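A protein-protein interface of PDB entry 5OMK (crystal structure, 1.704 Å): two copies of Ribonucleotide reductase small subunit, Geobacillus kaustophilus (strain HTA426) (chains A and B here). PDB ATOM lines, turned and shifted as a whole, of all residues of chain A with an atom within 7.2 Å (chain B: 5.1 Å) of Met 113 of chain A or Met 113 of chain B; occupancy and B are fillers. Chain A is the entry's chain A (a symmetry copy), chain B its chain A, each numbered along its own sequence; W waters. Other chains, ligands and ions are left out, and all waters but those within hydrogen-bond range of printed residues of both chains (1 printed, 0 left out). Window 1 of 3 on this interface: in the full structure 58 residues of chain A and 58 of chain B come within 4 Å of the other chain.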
ATOM      1  N   VAL A  86      -8.096 -21.217 -18.335  1.00  0.00           N
ATOM      2  CA  VAL A  86      -7.608 -19.842 -18.146  1.00  0.00           C
ATOM      3  C   VAL A  86      -8.128 -19.212 -16.846  1.00  0.00           C
ATOM      4  O   VAL A  86      -7.442 -18.372 -16.250  1.00  0.00           O
ATOM      5  CB  VAL A  86      -7.950 -18.957 -19.371  1.00  0.00           C
ATOM      6  CG1 VAL A  86      -7.275 -19.493 -20.600  1.00  0.00           C
ATOM      7  CG2 VAL A  86      -9.453 -18.824 -19.575  1.00  0.00           C
ATOM      8  N   THR A  87      -9.336 -19.555 -16.387  1.00  0.00           N
ATOM      9  CA  THR A  87      -9.762 -19.062 -15.071  1.00  0.00           C
ATOM     10  C   THR A  87      -8.765 -19.463 -13.978  1.00  0.00           C
ATOM     11  O   THR A  87      -8.330 -18.629 -13.173  1.00  0.00           O
ATOM     12  CB  THR A  87     -11.160 -19.580 -14.708  1.00  0.00           C
ATOM     13  OG1 THR A  87     -12.107 -19.131 -15.670  1.00  0.00           O
ATOM     14  CG2 THR A  87     -11.616 -19.003 -13.365  1.00  0.00           C
ATOM     15  N   ILE A  90      -4.735 -17.998 -14.723  1.00  0.00           N
ATOM     16  CA  ILE A  90      -4.286 -16.614 -14.661  1.00  0.00           C
ATOM     17  C   ILE A  90      -3.778 -16.273 -13.265  1.00  0.00           C
ATOM     18  O   ILE A  90      -3.025 -15.297 -13.102  1.00  0.00           O
ATOM     19  CB  ILE A  90      -5.405 -15.676 -15.136  1.00  0.00           C
ATOM     20  CG1 ILE A  90      -4.913 -14.225 -15.329  1.00  0.00           C
ATOM     21  CG2 ILE A  90      -6.573 -15.674 -14.171  1.00  0.00           C
ATOM     22  CD1 ILE A  90      -3.842 -14.059 -16.409  1.00  0.00           C
ATOM     23  N   LEU A  91      -4.147 -17.067 -12.253  1.00  0.00           N
ATOM     24  CA  LEU A  91      -3.780 -16.729 -10.873  1.00  0.00           C
ATOM     25  C   LEU A  91      -2.269 -16.543 -10.669  1.00  0.00           C
ATOM     26  O   LEU A  91      -1.897 -15.578  -9.986  1.00  0.00           O
ATOM     27  CB  LEU A  91      -4.356 -17.777  -9.910  1.00  0.00           C
ATOM     28  CG  LEU A  91      -5.895 -17.764  -9.710  1.00  0.00           C
ATOM     29  CD1 LEU A  91      -6.329 -18.969  -8.935  1.00  0.00           C
ATOM     30  CD2 LEU A  91      -6.290 -16.508  -8.979  1.00  0.00           C
ATOM     31  N   PRO A  92      -1.370 -17.391 -11.204  1.00  0.00           N
ATOM     32  CA  PRO A  92       0.072 -17.138 -11.037  1.00  0.00           C
ATOM     33  C   PRO A  92       0.551 -15.833 -11.660  1.00  0.00           C
ATOM     34  O   PRO A  92       1.498 -15.225 -11.136  1.00  0.00           O
ATOM     35  CB  PRO A  92       0.740 -18.340 -11.712  1.00  0.00           C
ATOM     36  CG  PRO A  92      -0.346 -19.370 -11.953  1.00  0.00           C
ATOM     37  CD  PRO A  92      -1.664 -18.654 -11.905  1.00  0.00           C
ATOM     38  N   ALA A  94      -1.297 -12.999 -11.888  1.00  0.00           N
ATOM     39  CA  ALA A  94      -1.713 -12.010 -10.902  1.00  0.00           C
ATOM     40  C   ALA A  94      -0.755 -11.991  -9.717  1.00  0.00           C
ATOM     41  O   ALA A  94      -0.352 -10.918  -9.246  1.00  0.00           O
ATOM     42  CB  ALA A  94      -3.139 -12.317 -10.432  1.00  0.00           C
ATOM     43  N   HIS A  95      -0.417 -13.178  -9.188  1.00  0.00           N
ATOM     44  CA  HIS A  95       0.551 -13.264  -8.098  1.00  0.00           C
ATOM     45  C   HIS A  95       1.891 -12.631  -8.456  1.00  0.00           C
ATOM     46  O   HIS A  95       2.459 -11.848  -7.670  1.00  0.00           O
ATOM     47  CB  HIS A  95       0.786 -14.713  -7.698  1.00  0.00           C
ATOM     48  CG  HIS A  95       1.976 -14.892  -6.815  1.00  0.00           C
ATOM     49  ND1 HIS A  95       1.908 -14.744  -5.447  1.00  0.00           N
ATOM     50  CD2 HIS A  95       3.265 -15.192  -7.105  1.00  0.00           C
ATOM     51  CE1 HIS A  95       3.098 -14.974  -4.931  1.00  0.00           C
ATOM     52  NE2 HIS A  95       3.937 -15.244  -5.916  1.00  0.00           N
ATOM     53  N   VAL A 106      -2.546  -5.601 -11.344  1.00  0.00           N
ATOM     54  CA  VAL A 106      -3.357  -6.463 -10.480  1.00  0.00           C
ATOM     55  C   VAL A 106      -4.815  -6.024 -10.501  1.00  0.00           C
ATOM     56  O   VAL A 106      -5.707  -6.855 -10.648  1.00  0.00           O
ATOM     57  CB  VAL A 106      -2.785  -6.494  -9.044  1.00  0.00           C
ATOM     58  CG1 VAL A 106      -3.708  -7.296  -8.088  1.00  0.00           C
ATOM     59  CG2 VAL A 106      -1.345  -7.076  -9.063  1.00  0.00           C
ATOM     60  N   LEU A 107      -5.078  -4.717 -10.354  1.00  0.00           N
ATOM     61  CA  LEU A 107      -6.457  -4.235 -10.421  1.00  0.00           C
ATOM     62  C   LEU A 107      -7.114  -4.705 -11.716  1.00  0.00           C
ATOM     63  O   LEU A 107      -8.197  -5.291 -11.704  1.00  0.00           O
ATOM     64  CB  LEU A 107      -6.509  -2.712 -10.320  1.00  0.00           C
ATOM     65  CG  LEU A 107      -5.938  -2.003  -9.100  1.00  0.00           C
ATOM     66  CD1 LEU A 107      -6.105  -0.443  -9.197  1.00  0.00           C
ATOM     67  CD2 LEU A 107      -6.534  -2.511  -7.826  1.00  0.00           C
ATOM     68  N   PHE A 108      -6.418  -4.546 -12.835  1.00  0.00           N
ATOM     69  CA  PHE A 108      -6.982  -4.991 -14.095  1.00  0.00           C
ATOM     70  C   PHE A 108      -7.166  -6.502 -14.106  1.00  0.00           C
ATOM     71  O   PHE A 108      -8.183  -7.006 -14.597  1.00  0.00           O
ATOM     72  CB  PHE A 108      -6.123  -4.579 -15.290  1.00  0.00           C
ATOM     73  CG  PHE A 108      -6.528  -5.338 -16.521  1.00  0.00           C
ATOM     74  CD1 PHE A 108      -7.737  -5.045 -17.137  1.00  0.00           C
ATOM     75  CD2 PHE A 108      -5.806  -6.453 -16.940  1.00  0.00           C
ATOM     76  CE1 PHE A 108      -8.196  -5.802 -18.174  1.00  0.00           C
ATOM     77  CE2 PHE A 108      -6.250  -7.213 -18.005  1.00  0.00           C
ATOM     78  CZ  PHE A 108      -7.445  -6.855 -18.633  1.00  0.00           C
ATOM     79  N   LEU A 109      -6.175  -7.252 -13.598  1.00  0.00           N
ATOM     80  CA  LEU A 109      -6.302  -8.699 -13.637  1.00  0.00           C
ATOM     81  C   LEU A 109      -7.488  -9.204 -12.830  1.00  0.00           C
ATOM     82  O   LEU A 109      -7.974 -10.287 -13.152  1.00  0.00           O
ATOM     83  CB  LEU A 109      -5.019  -9.378 -13.175  1.00  0.00           C
ATOM     84  CG  LEU A 109      -3.927  -9.333 -14.265  1.00  0.00           C
ATOM     85  CD1 LEU A 109      -2.604  -9.832 -13.758  1.00  0.00           C
ATOM     86  CD2 LEU A 109      -4.256 -10.163 -15.510  1.00  0.00           C
ATOM     87  N   THR A 110      -7.987  -8.459 -11.835  1.00  0.00           N
ATOM     88  CA  THR A 110      -9.227  -8.879 -11.168  1.00  0.00           C
ATOM     89  C   THR A 110     -10.403  -8.900 -12.144  1.00  0.00           C
ATOM     90  O   THR A 110     -11.274  -9.774 -12.027  1.00  0.00           O
ATOM     91  CB  THR A 110      -9.597  -8.024  -9.938  1.00  0.00           C
ATOM     92  OG1 THR A 110     -10.069  -6.708 -10.289  1.00  0.00           O
ATOM     93  CG2 THR A 110      -8.442  -7.883  -8.974  1.00  0.00           C
ATOM     94  N   THR A 111     -10.428  -7.993 -13.132  1.00  0.00           N
ATOM     95  CA  THR A 111     -11.515  -8.015 -14.107  1.00  0.00           C
ATOM     96  C   THR A 111     -11.323  -9.153 -15.100  1.00  0.00           C
ATOM     97  O   THR A 111     -12.295  -9.801 -15.512  1.00  0.00           O
ATOM     98  CB  THR A 111     -11.653  -6.670 -14.863  1.00  0.00           C
ATOM     99  OG1 THR A 111     -10.592  -6.484 -15.810  1.00  0.00           O
ATOM    100  CG2 THR A 111     -11.734  -5.523 -13.912  1.00  0.00           C
ATOM    101  N   PHE A 112     -10.065  -9.397 -15.478  1.00  0.00           N
ATOM    102  CA  PHE A 112      -9.705 -10.516 -16.337  1.00  0.00           C
ATOM    103  C   PHE A 112     -10.201 -11.846 -15.745  1.00  0.00           C
ATOM    104  O   PHE A 112     -10.894 -12.626 -16.413  1.00  0.00           O
ATOM    105  CB  PHE A 112      -8.170 -10.488 -16.493  1.00  0.00           C
ATOM    106  CG  PHE A 112      -7.598 -11.293 -17.643  1.00  0.00           C
ATOM    107  CD1 PHE A 112      -6.490 -10.807 -18.326  1.00  0.00           C
ATOM    108  CD2 PHE A 112      -8.060 -12.539 -17.975  1.00  0.00           C
ATOM    109  CE1 PHE A 112      -5.914 -11.509 -19.363  1.00  0.00           C
ATOM    110  CE2 PHE A 112      -7.475 -13.264 -19.003  1.00  0.00           C
ATOM    111  CZ  PHE A 112      -6.400 -12.761 -19.693  1.00  0.00           C
ATOM    112  N   MET A 113      -9.826 -12.116 -14.498  1.00  0.00           N
ATOM    113  CA  MET A 113     -10.233 -13.349 -13.816  1.00  0.00           C
ATOM    114  C   MET A 113     -11.743 -13.483 -13.757  1.00  0.00           C
ATOM    115  O   MET A 113     -12.305 -14.545 -14.069  1.00  0.00           O
ATOM    116  CB  MET A 113      -9.629 -13.366 -12.410  1.00  0.00           C
ATOM    117  CG  MET A 113      -8.137 -13.488 -12.487  1.00  0.00           C
ATOM    118  SD  MET A 113      -7.141 -13.512 -10.963  1.00  0.00           S
ATOM    119  CE  MET A 113      -7.832 -12.170 -10.078  1.00  0.00           C
ATOM    120  N   HIS A 114     -12.422 -12.402 -13.380  1.00  0.00           N
ATOM    121  CA  HIS A 114     -13.874 -12.444 -13.285  1.00  0.00           C
ATOM    122  C   HIS A 114     -14.523 -12.637 -14.652  1.00  0.00           C
ATOM    123  O   HIS A 114     -15.518 -13.373 -14.779  1.00  0.00           O
ATOM    124  CB  HIS A 114     -14.425 -11.183 -12.618  1.00  0.00           C
ATOM    125  CG  HIS A 114     -15.909 -11.235 -12.486  1.00  0.00           C
ATOM    126  ND1 HIS A 114     -16.531 -12.263 -11.808  1.00  0.00           N
ATOM    127  CD2 HIS A 114     -16.899 -10.453 -12.986  1.00  0.00           C
ATOM    128  CE1 HIS A 114     -17.844 -12.096 -11.870  1.00  0.00           C
ATOM    129  NE2 HIS A 114     -18.095 -11.006 -12.571  1.00  0.00           N
ATOM    130  N   ASP A 115     -13.957 -12.029 -15.698  1.00  0.00           N
ATOM    131  CA  ASP A 115     -14.447 -12.286 -17.051  1.00  0.00           C
ATOM    132  C   ASP A 115     -14.418 -13.793 -17.352  1.00  0.00           C
ATOM    133  O   ASP A 115     -15.388 -14.377 -17.877  1.00  0.00           O
ATOM    134  CB  ASP A 115     -13.561 -11.591 -18.093  1.00  0.00           C
ATOM    135  CG  ASP A 115     -13.720 -10.091 -18.170  1.00  0.00           C
ATOM    136  OD1 ASP A 115     -14.636  -9.495 -17.597  1.00  0.00           O
ATOM    137  OD2 ASP A 115     -12.839  -9.473 -18.815  1.00  0.00           O
ATOM    138  N   GLU A 116     -13.269 -14.427 -17.091  1.00  0.00           N
ATOM    139  CA  GLU A 116     -13.126 -15.838 -17.428  1.00  0.00           C
ATOM    140  C   GLU A 116     -14.088 -16.697 -16.632  1.00  0.00           C
ATOM    141  O   GLU A 116     -14.633 -17.666 -17.175  1.00  0.00           O
ATOM    142  CB  GLU A 116     -11.680 -16.297 -17.213  1.00  0.00           C
ATOM    143  CG  GLU A 116     -10.635 -15.550 -18.044  1.00  0.00           C
ATOM    144  CD  GLU A 116     -10.791 -15.717 -19.576  1.00  0.00           C
ATOM    145  OE1 GLU A 116      -9.865 -15.296 -20.293  1.00  0.00           O
ATOM    146  OE2 GLU A 116     -11.782 -16.296 -20.065  1.00  0.00           O
ATOM    147  N   ALA A 117     -14.322 -16.367 -15.346  1.00  0.00           N
ATOM    148  CA  ALA A 117     -15.354 -17.053 -14.558  1.00  0.00           C
ATOM    149  C   ALA A 117     -16.727 -16.969 -15.223  1.00  0.00           C
ATOM    150  O   ALA A 117     -17.461 -17.981 -15.328  1.00  0.00           O
ATOM    151  CB  ALA A 117     -15.425 -16.475 -13.146  1.00  0.00           C
ATOM    152  N   LYS A 118     -17.100 -15.777 -15.681  1.00  0.00           N
ATOM    153  CA  LYS A 118     -18.360 -15.637 -16.412  1.00  0.00           C
ATOM    154  C   LYS A 118     -18.330 -16.447 -17.707  1.00  0.00           C
ATOM    155  O   LYS A 118     -19.354 -17.000 -18.114  1.00  0.00           O
ATOM    156  CB  LYS A 118     -18.665 -14.155 -16.703  1.00  0.00           C
ATOM    157  CG  LYS A 118     -18.900 -13.307 -15.454  1.00  0.00           C
ATOM    158  CD  LYS A 118     -19.444 -11.889 -15.789  1.00  0.00           C
ATOM    159  CE  LYS A 118     -18.527 -11.122 -16.664  1.00  0.00           C
ATOM    160  NZ  LYS A 118     -19.146  -9.798 -16.901  1.00  0.00           N
ATOM    161  N   HIS A 119     -17.176 -16.556 -18.368  1.00  0.00           N
ATOM    162  CA  HIS A 119     -17.139 -17.361 -19.591  1.00  0.00           C
ATOM    163  C   HIS A 119     -17.378 -18.836 -19.282  1.00  0.00           C
ATOM    164  O   HIS A 119     -18.107 -19.522 -20.012  1.00  0.00           O
ATOM    165  CB  HIS A 119     -15.803 -17.233 -20.318  1.00  0.00           C
ATOM    166  CG  HIS A 119     -15.459 -15.846 -20.733  1.00  0.00           C
ATOM    167  ND1 HIS A 119     -14.250 -15.516 -21.320  1.00  0.00           N
ATOM    168  CD2 HIS A 119     -16.148 -14.695 -20.605  1.00  0.00           C
ATOM    169  CE1 HIS A 119     -14.242 -14.218 -21.576  1.00  0.00           C
ATOM    170  NE2 HIS A 119     -15.358 -13.689 -21.103  1.00  0.00           N
ATOM    171  N   TYR A 176      -0.650 -17.833 -23.131  1.00  0.00           N
ATOM    172  CA  TYR A 176      -2.005 -17.546 -22.653  1.00  0.00           C
ATOM    173  C   TYR A 176      -2.682 -16.501 -23.540  1.00  0.00           C
ATOM    174  O   TYR A 176      -3.726 -16.752 -24.146  1.00  0.00           O
ATOM    175  CB  TYR A 176      -1.929 -17.065 -21.198  1.00  0.00           C
ATOM    176  CG  TYR A 176      -3.217 -16.881 -20.466  1.00  0.00           C
ATOM    177  CD1 TYR A 176      -3.358 -17.392 -19.190  1.00  0.00           C
ATOM    178  CD2 TYR A 176      -4.286 -16.188 -21.019  1.00  0.00           C
ATOM    179  CE1 TYR A 176      -4.523 -17.247 -18.479  1.00  0.00           C
ATOM    180  CE2 TYR A 176      -5.485 -16.033 -20.315  1.00  0.00           C
ATOM    181  CZ  TYR A 176      -5.582 -16.555 -19.028  1.00  0.00           C
ATOM    182  OH  TYR A 176      -6.731 -16.423 -18.261  1.00  0.00           O
ATOM    183  N   HIS A 219      -8.287  -8.832 -22.713  1.00  0.00           N
ATOM    184  CA  HIS A 219      -7.335  -9.893 -22.357  1.00  0.00           C
ATOM    185  C   HIS A 219      -6.126  -9.868 -23.284  1.00  0.00           C
ATOM    186  O   HIS A 219      -4.973  -9.948 -22.840  1.00  0.00           O
ATOM    187  CB  HIS A 219      -8.045 -11.270 -22.430  1.00  0.00           C
ATOM    188  CG  HIS A 219      -9.253 -11.350 -21.567  1.00  0.00           C
ATOM    189  ND1 HIS A 219     -10.047 -12.486 -21.475  1.00  0.00           N
ATOM    190  CD2 HIS A 219      -9.845 -10.412 -20.788  1.00  0.00           C
ATOM    191  CE1 HIS A 219     -11.058 -12.233 -20.657  1.00  0.00           C
ATOM    192  NE2 HIS A 219     -10.954 -10.991 -20.224  1.00  0.00           N
ATOM    193  N   THR B  87      -6.404  -7.151  -1.308  1.00  0.00           N
ATOM    194  CA  THR B  87      -6.387  -7.385  -2.758  1.00  0.00           C
ATOM    195  C   THR B  87      -5.251  -8.335  -3.153  1.00  0.00           C
ATOM    196  O   THR B  87      -5.461  -9.312  -3.885  1.00  0.00           O
ATOM    197  CB  THR B  87      -6.250  -6.068  -3.533  1.00  0.00           C
ATOM    198  OG1 THR B  87      -7.353  -5.218  -3.241  1.00  0.00           O
ATOM    199  CG2 THR B  87      -6.300  -6.323  -5.042  1.00  0.00           C
ATOM    200  N   ILE B  90      -5.492 -12.202  -1.170  1.00  0.00           N
ATOM    201  CA  ILE B  90      -6.481 -13.243  -1.408  1.00  0.00           C
ATOM    202  C   ILE B  90      -5.997 -14.213  -2.480  1.00  0.00           C
ATOM    203  O   ILE B  90      -6.501 -15.346  -2.562  1.00  0.00           O
ATOM    204  CB  ILE B  90      -7.840 -12.610  -1.743  1.00  0.00           C
ATOM    205  CG1 ILE B  90      -8.983 -13.650  -1.763  1.00  0.00           C
ATOM    206  CG2 ILE B  90      -7.804 -11.895  -3.079  1.00  0.00           C
ATOM    207  CD1 ILE B  90      -9.241 -14.330  -0.417  1.00  0.00           C
ATOM    208  N   LEU B  91      -5.012 -13.810  -3.291  1.00  0.00           N
ATOM    209  CA  LEU B  91      -4.578 -14.654  -4.409  1.00  0.00           C
ATOM    210  C   LEU B  91      -4.153 -16.067  -3.980  1.00  0.00           C
ATOM    211  O   LEU B  91      -4.547 -17.018  -4.670  1.00  0.00           O
ATOM    212  CB  LEU B  91      -3.468 -13.945  -5.198  1.00  0.00           C
ATOM    213  CG  LEU B  91      -3.894 -12.714  -6.040  1.00  0.00           C
ATOM    214  CD1 LEU B  91      -2.686 -11.998  -6.562  1.00  0.00           C
ATOM    215  CD2 LEU B  91      -4.761 -13.169  -7.184  1.00  0.00           C
ATOM    216  N   ALA B  94      -7.343 -18.206  -3.486  1.00  0.00           N
ATOM    217  CA  ALA B  94      -7.882 -18.590  -4.785  1.00  0.00           C
ATOM    218  C   ALA B  94      -7.073 -19.729  -5.392  1.00  0.00           C
ATOM    219  O   ALA B  94      -7.639 -20.699  -5.915  1.00  0.00           O
ATOM    220  CB  ALA B  94      -7.885 -17.377  -5.722  1.00  0.00           C
ATOM    221  N   LEU B 109     -14.502 -16.324  -5.711  1.00  0.00           N
ATOM    222  CA  LEU B 109     -13.345 -15.530  -5.335  1.00  0.00           C
ATOM    223  C   LEU B 109     -12.957 -14.520  -6.403  1.00  0.00           C
ATOM    224  O   LEU B 109     -12.345 -13.516  -6.039  1.00  0.00           O
ATOM    225  CB  LEU B 109     -12.156 -16.418  -4.989  1.00  0.00           C
ATOM    226  CG  LEU B 109     -12.310 -17.057  -3.593  1.00  0.00           C
ATOM    227  CD1 LEU B 109     -11.241 -18.075  -3.318  1.00  0.00           C
ATOM    228  CD2 LEU B 109     -12.260 -16.051  -2.439  1.00  0.00           C
ATOM    229  N   THR B 110     -13.315 -14.722  -7.678  1.00  0.00           N
ATOM    230  CA  THR B 110     -13.077 -13.666  -8.672  1.00  0.00           C
ATOM    231  C   THR B 110     -13.865 -12.401  -8.338  1.00  0.00           C
ATOM    232  O   THR B 110     -13.364 -11.292  -8.577  1.00  0.00           O
ATOM    233  CB  THR B 110     -13.383 -14.094 -10.124  1.00  0.00           C
ATOM    234  OG1 THR B 110     -14.794 -14.216 -10.388  1.00  0.00           O
ATOM    235  CG2 THR B 110     -12.708 -15.394 -10.489  1.00  0.00           C
ATOM    236  N   THR B 111     -15.064 -12.532  -7.750  1.00  0.00           N
ATOM    237  CA  THR B 111     -15.822 -11.341  -7.379  1.00  0.00           C
ATOM    238  C   THR B 111     -15.234 -10.698  -6.131  1.00  0.00           C
ATOM    239  O   THR B 111     -15.184  -9.464  -6.021  1.00  0.00           O
ATOM    240  CB  THR B 111     -17.325 -11.646  -7.159  1.00  0.00           C
ATOM    241  OG1 THR B 111     -17.546 -12.365  -5.937  1.00  0.00           O
ATOM    242  CG2 THR B 111     -17.903 -12.375  -8.325  1.00  0.00           C
ATOM    243  N   PHE B 112     -14.783 -11.536  -5.194  1.00  0.00           N
ATOM    244  CA  PHE B 112     -14.097 -11.080  -3.994  1.00  0.00           C
ATOM    245  C   PHE B 112     -12.885 -10.204  -4.351  1.00  0.00           C
ATOM    246  O   PHE B 112     -12.745  -9.074  -3.864  1.00  0.00           O
ATOM    247  CB  PHE B 112     -13.688 -12.341  -3.202  1.00  0.00           C
ATOM    248  CG  PHE B 112     -13.324 -12.129  -1.745  1.00  0.00           C
ATOM    249  CD1 PHE B 112     -13.667 -13.099  -0.812  1.00  0.00           C
ATOM    250  CD2 PHE B 112     -12.571 -11.067  -1.319  1.00  0.00           C
ATOM    251  CE1 PHE B 112     -13.339 -12.970   0.520  1.00  0.00           C
ATOM    252  CE2 PHE B 112     -12.217 -10.936   0.016  1.00  0.00           C
ATOM    253  CZ  PHE B 112     -12.589 -11.886   0.936  1.00  0.00           C
ATOM    254  N   MET B 113     -11.995 -10.736  -5.184  1.00  0.00           N
ATOM    255  CA  MET B 113     -10.797 -10.005  -5.608  1.00  0.00           C
ATOM    256  C   MET B 113     -11.151  -8.689  -6.277  1.00  0.00           C
ATOM    257  O   MET B 113     -10.576  -7.635  -5.960  1.00  0.00           O
ATOM    258  CB  MET B 113      -9.976 -10.891  -6.549  1.00  0.00           C
ATOM    259  CG  MET B 113      -9.421 -12.066  -5.802  1.00  0.00           C
ATOM    260  SD  MET B 113      -8.415 -13.310  -6.672  1.00  0.00           S
ATOM    261  CE  MET B 113      -9.385 -13.600  -8.100  1.00  0.00           C
ATOM    262  N   HIS B 114     -12.117  -8.728  -7.191  1.00  0.00           N
ATOM    263  CA  HIS B 114     -12.513  -7.514  -7.890  1.00  0.00           C
ATOM    264  C   HIS B 114     -13.155  -6.503  -6.945  1.00  0.00           C
ATOM    265  O   HIS B 114     -12.916  -5.288  -7.065  1.00  0.00           O
ATOM    266  CB  HIS B 114     -13.464  -7.824  -9.048  1.00  0.00           C
ATOM    267  CG  HIS B 114     -13.846  -6.589  -9.790  1.00  0.00           C
ATOM    268  ND1 HIS B 114     -12.891  -5.772 -10.360  1.00  0.00           N
ATOM    269  CD2 HIS B 114     -15.042  -5.985 -10.005  1.00  0.00           C
ATOM    270  CE1 HIS B 114     -13.486  -4.729 -10.921  1.00  0.00           C
ATOM    271  NE2 HIS B 114     -14.788  -4.836 -10.727  1.00  0.00           N
ATOM    272  N   ASP B 115     -13.935  -6.976  -5.969  1.00  0.00           N
ATOM    273  CA  ASP B 115     -14.464  -6.072  -4.949  1.00  0.00           C
ATOM    274  C   ASP B 115     -13.319  -5.310  -4.265  1.00  0.00           C
ATOM    275  O   ASP B 115     -13.373  -4.077  -4.074  1.00  0.00           O
ATOM    276  CB  ASP B 115     -15.212  -6.856  -3.861  1.00  0.00           C
ATOM    277  CG  ASP B 115     -16.557  -7.402  -4.277  1.00  0.00           C
ATOM    278  OD1 ASP B 115     -17.108  -7.068  -5.329  1.00  0.00           O
ATOM    279  OD2 ASP B 115     -17.069  -8.255  -3.511  1.00  0.00           O
ATOM    280  N   GLU B 116     -12.300  -6.050  -3.817  1.00  0.00           N
ATOM    281  CA  GLU B 116     -11.214  -5.418  -3.078  1.00  0.00           C
ATOM    282  C   GLU B 116     -10.460  -4.426  -3.942  1.00  0.00           C
ATOM    283  O   GLU B 116     -10.059  -3.367  -3.446  1.00  0.00           O
ATOM    284  CB  GLU B 116     -10.263  -6.478  -2.510  1.00  0.00           C
ATOM    285  CG  GLU B 116     -10.911  -7.476  -1.549  1.00  0.00           C
ATOM    286  CD  GLU B 116     -11.485  -6.846  -0.256  1.00  0.00           C
ATOM    287  OE1 GLU B 116     -11.847  -7.625   0.646  1.00  0.00           O
ATOM    288  OE2 GLU B 116     -11.534  -5.609  -0.106  1.00  0.00           O
ATOM    289  N   ALA B 117     -10.256  -4.738  -5.238  1.00  0.00           N
ATOM    290  CA  ALA B 117      -9.675  -3.766  -6.173  1.00  0.00           C
ATOM    291  C   ALA B 117     -10.481  -2.470  -6.220  1.00  0.00           C
ATOM    292  O   ALA B 117      -9.916  -1.350  -6.170  1.00  0.00           O
ATOM    293  CB  ALA B 117      -9.572  -4.365  -7.574  1.00  0.00           C
HETATM  294  O   HOH W   1      -1.957 -17.100  -6.915  1.00  0.00           O
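Water W1 bridges O of Leu 91 of chain B (3.4 Å) and O of Leu 91 of chain A (3.4 Å).
Thr 110 of chain A touches Met 113 of chain B, and with the chains exchanged Met 113 of chain A touches Thr 110 of chain B. Thr 110 of chain A touches His 114 of chain B, and with the chains exchanged His 114 of chain A touches Thr 110 of chain B. Thr 111 of chain A touches His 114 of chain B, and with the chains exchanged His 114 of chain A touches Thr 111 of chain B. Met 113 of chain B touches its own counterpart, Met 113 of chain A. Of the 13 pairs that touch across the chains among the printed residues, 11 have their exchanged pair printed and touching as well.
The backbone carbonyl oxygen (O) of Leu 107 of chain A lies within hydrogen-bond range of the side-chain hydroxyl (OG1) of Thr 110 of chain A, 2.7 Å away. OG1 of Thr 111 of chain A lies within hydrogen-bond range of O of Phe 108 of chain A (2.7 Å).
Of the 13 printed residues of chain B, 7 touch a printed residue of chain A. Of the 23 printed residues of chain A, 9 touch a printed residue of chain B. Printed residues of chain A that touch a printed residue of chain B: Leu 91, Ala 94, His 95, Leu 107, Thr 110, Thr 111, Met 113, His 114 and Ala 117. Hydrophobic or aromatic side chains of chain A that line the printed part of chain B: Leu 91, Ala 94, Leu 107, Met 113, His 114 and Ala 117.
A ring nitrogen (ND1) of His 114 of chain A lies within hydrogen-bond range of the side-chain hydroxyl (OG1) of Thr 110 of chain B, at 3.0 Å. ND1 of His 114 of chain B sits at hydrogen-bond distance from OG1 of Thr 110 of chain A.
Of the printed residues of chain B, Met 113 of chain A touches Thr 110 (3.7 Å) and Met 113 (2.9 Å). Of the printed residues of chain A, Met 113 of chain B touches Thr 110 (3.7 Å) and Met 113 (2.9 Å). Of the printed residues of chain B, Leu 91 of chain A touches Ala 94. Of the printed residues of chain A, His 114 of chain B touches Thr 110 (3.0 Å) and Thr 111 (3.6 Å). Of the printed residues of chain A, Ala 94 of chain B touches Leu 91. Printed residues of chain B within 4 Å of Thr 110 of chain A: Met 113 (3.7 Å), His 114 (3.0 Å) and Ala 117 (3.6 Å). Printed residues of chain A within 4 Å of Ala 117 of chain B: Leu 107 (3.6 Å) and Thr 110 (3.6 Å). Phe 112 of chain A touches none of the printed residues of chain B. The nearest printed residue of chain A that does not touch Met 113 of chain B is Leu 91 of chain A (4.3 Å). The nearest printed residue of chain A that does not touch Thr 111 of chain B is Thr 110 of chain A (6.3 Å).
Leu 91 of chain A touches Ala 94 of chain B (CD1 to C, 3.7 Å). Ala 94 of chain A touches Leu 91 of chain B (C to CD1, 3.7 Å). His 95 of chain A touches Leu 91 of chain B (N to CD1, 3.7 Å). CB of Ala 117 of chain B touches CD2 of Leu 107 of chain A, 3.6 Å away. O of Met 113 of chain B touches CG2 of Thr 110 of chain A, at 3.7 Å. CB of Ala 117 of chain B touches OG1 of Thr 110 of chain A, at 3.6 Å. Thr 111 of chain A touches His 114 of chain B (CG2 to CE1, 3.6 Å). Met 113 of chain A touches Met 113 of chain B (CE to CE, 2.9 Å). Thr 111 of chain B touches His 114 of chain A (CG2 to CE1, 3.6 Å). Thr 110 of chain B touches Ala 117 of chain A (OG1 to CB, 3.6 Å).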
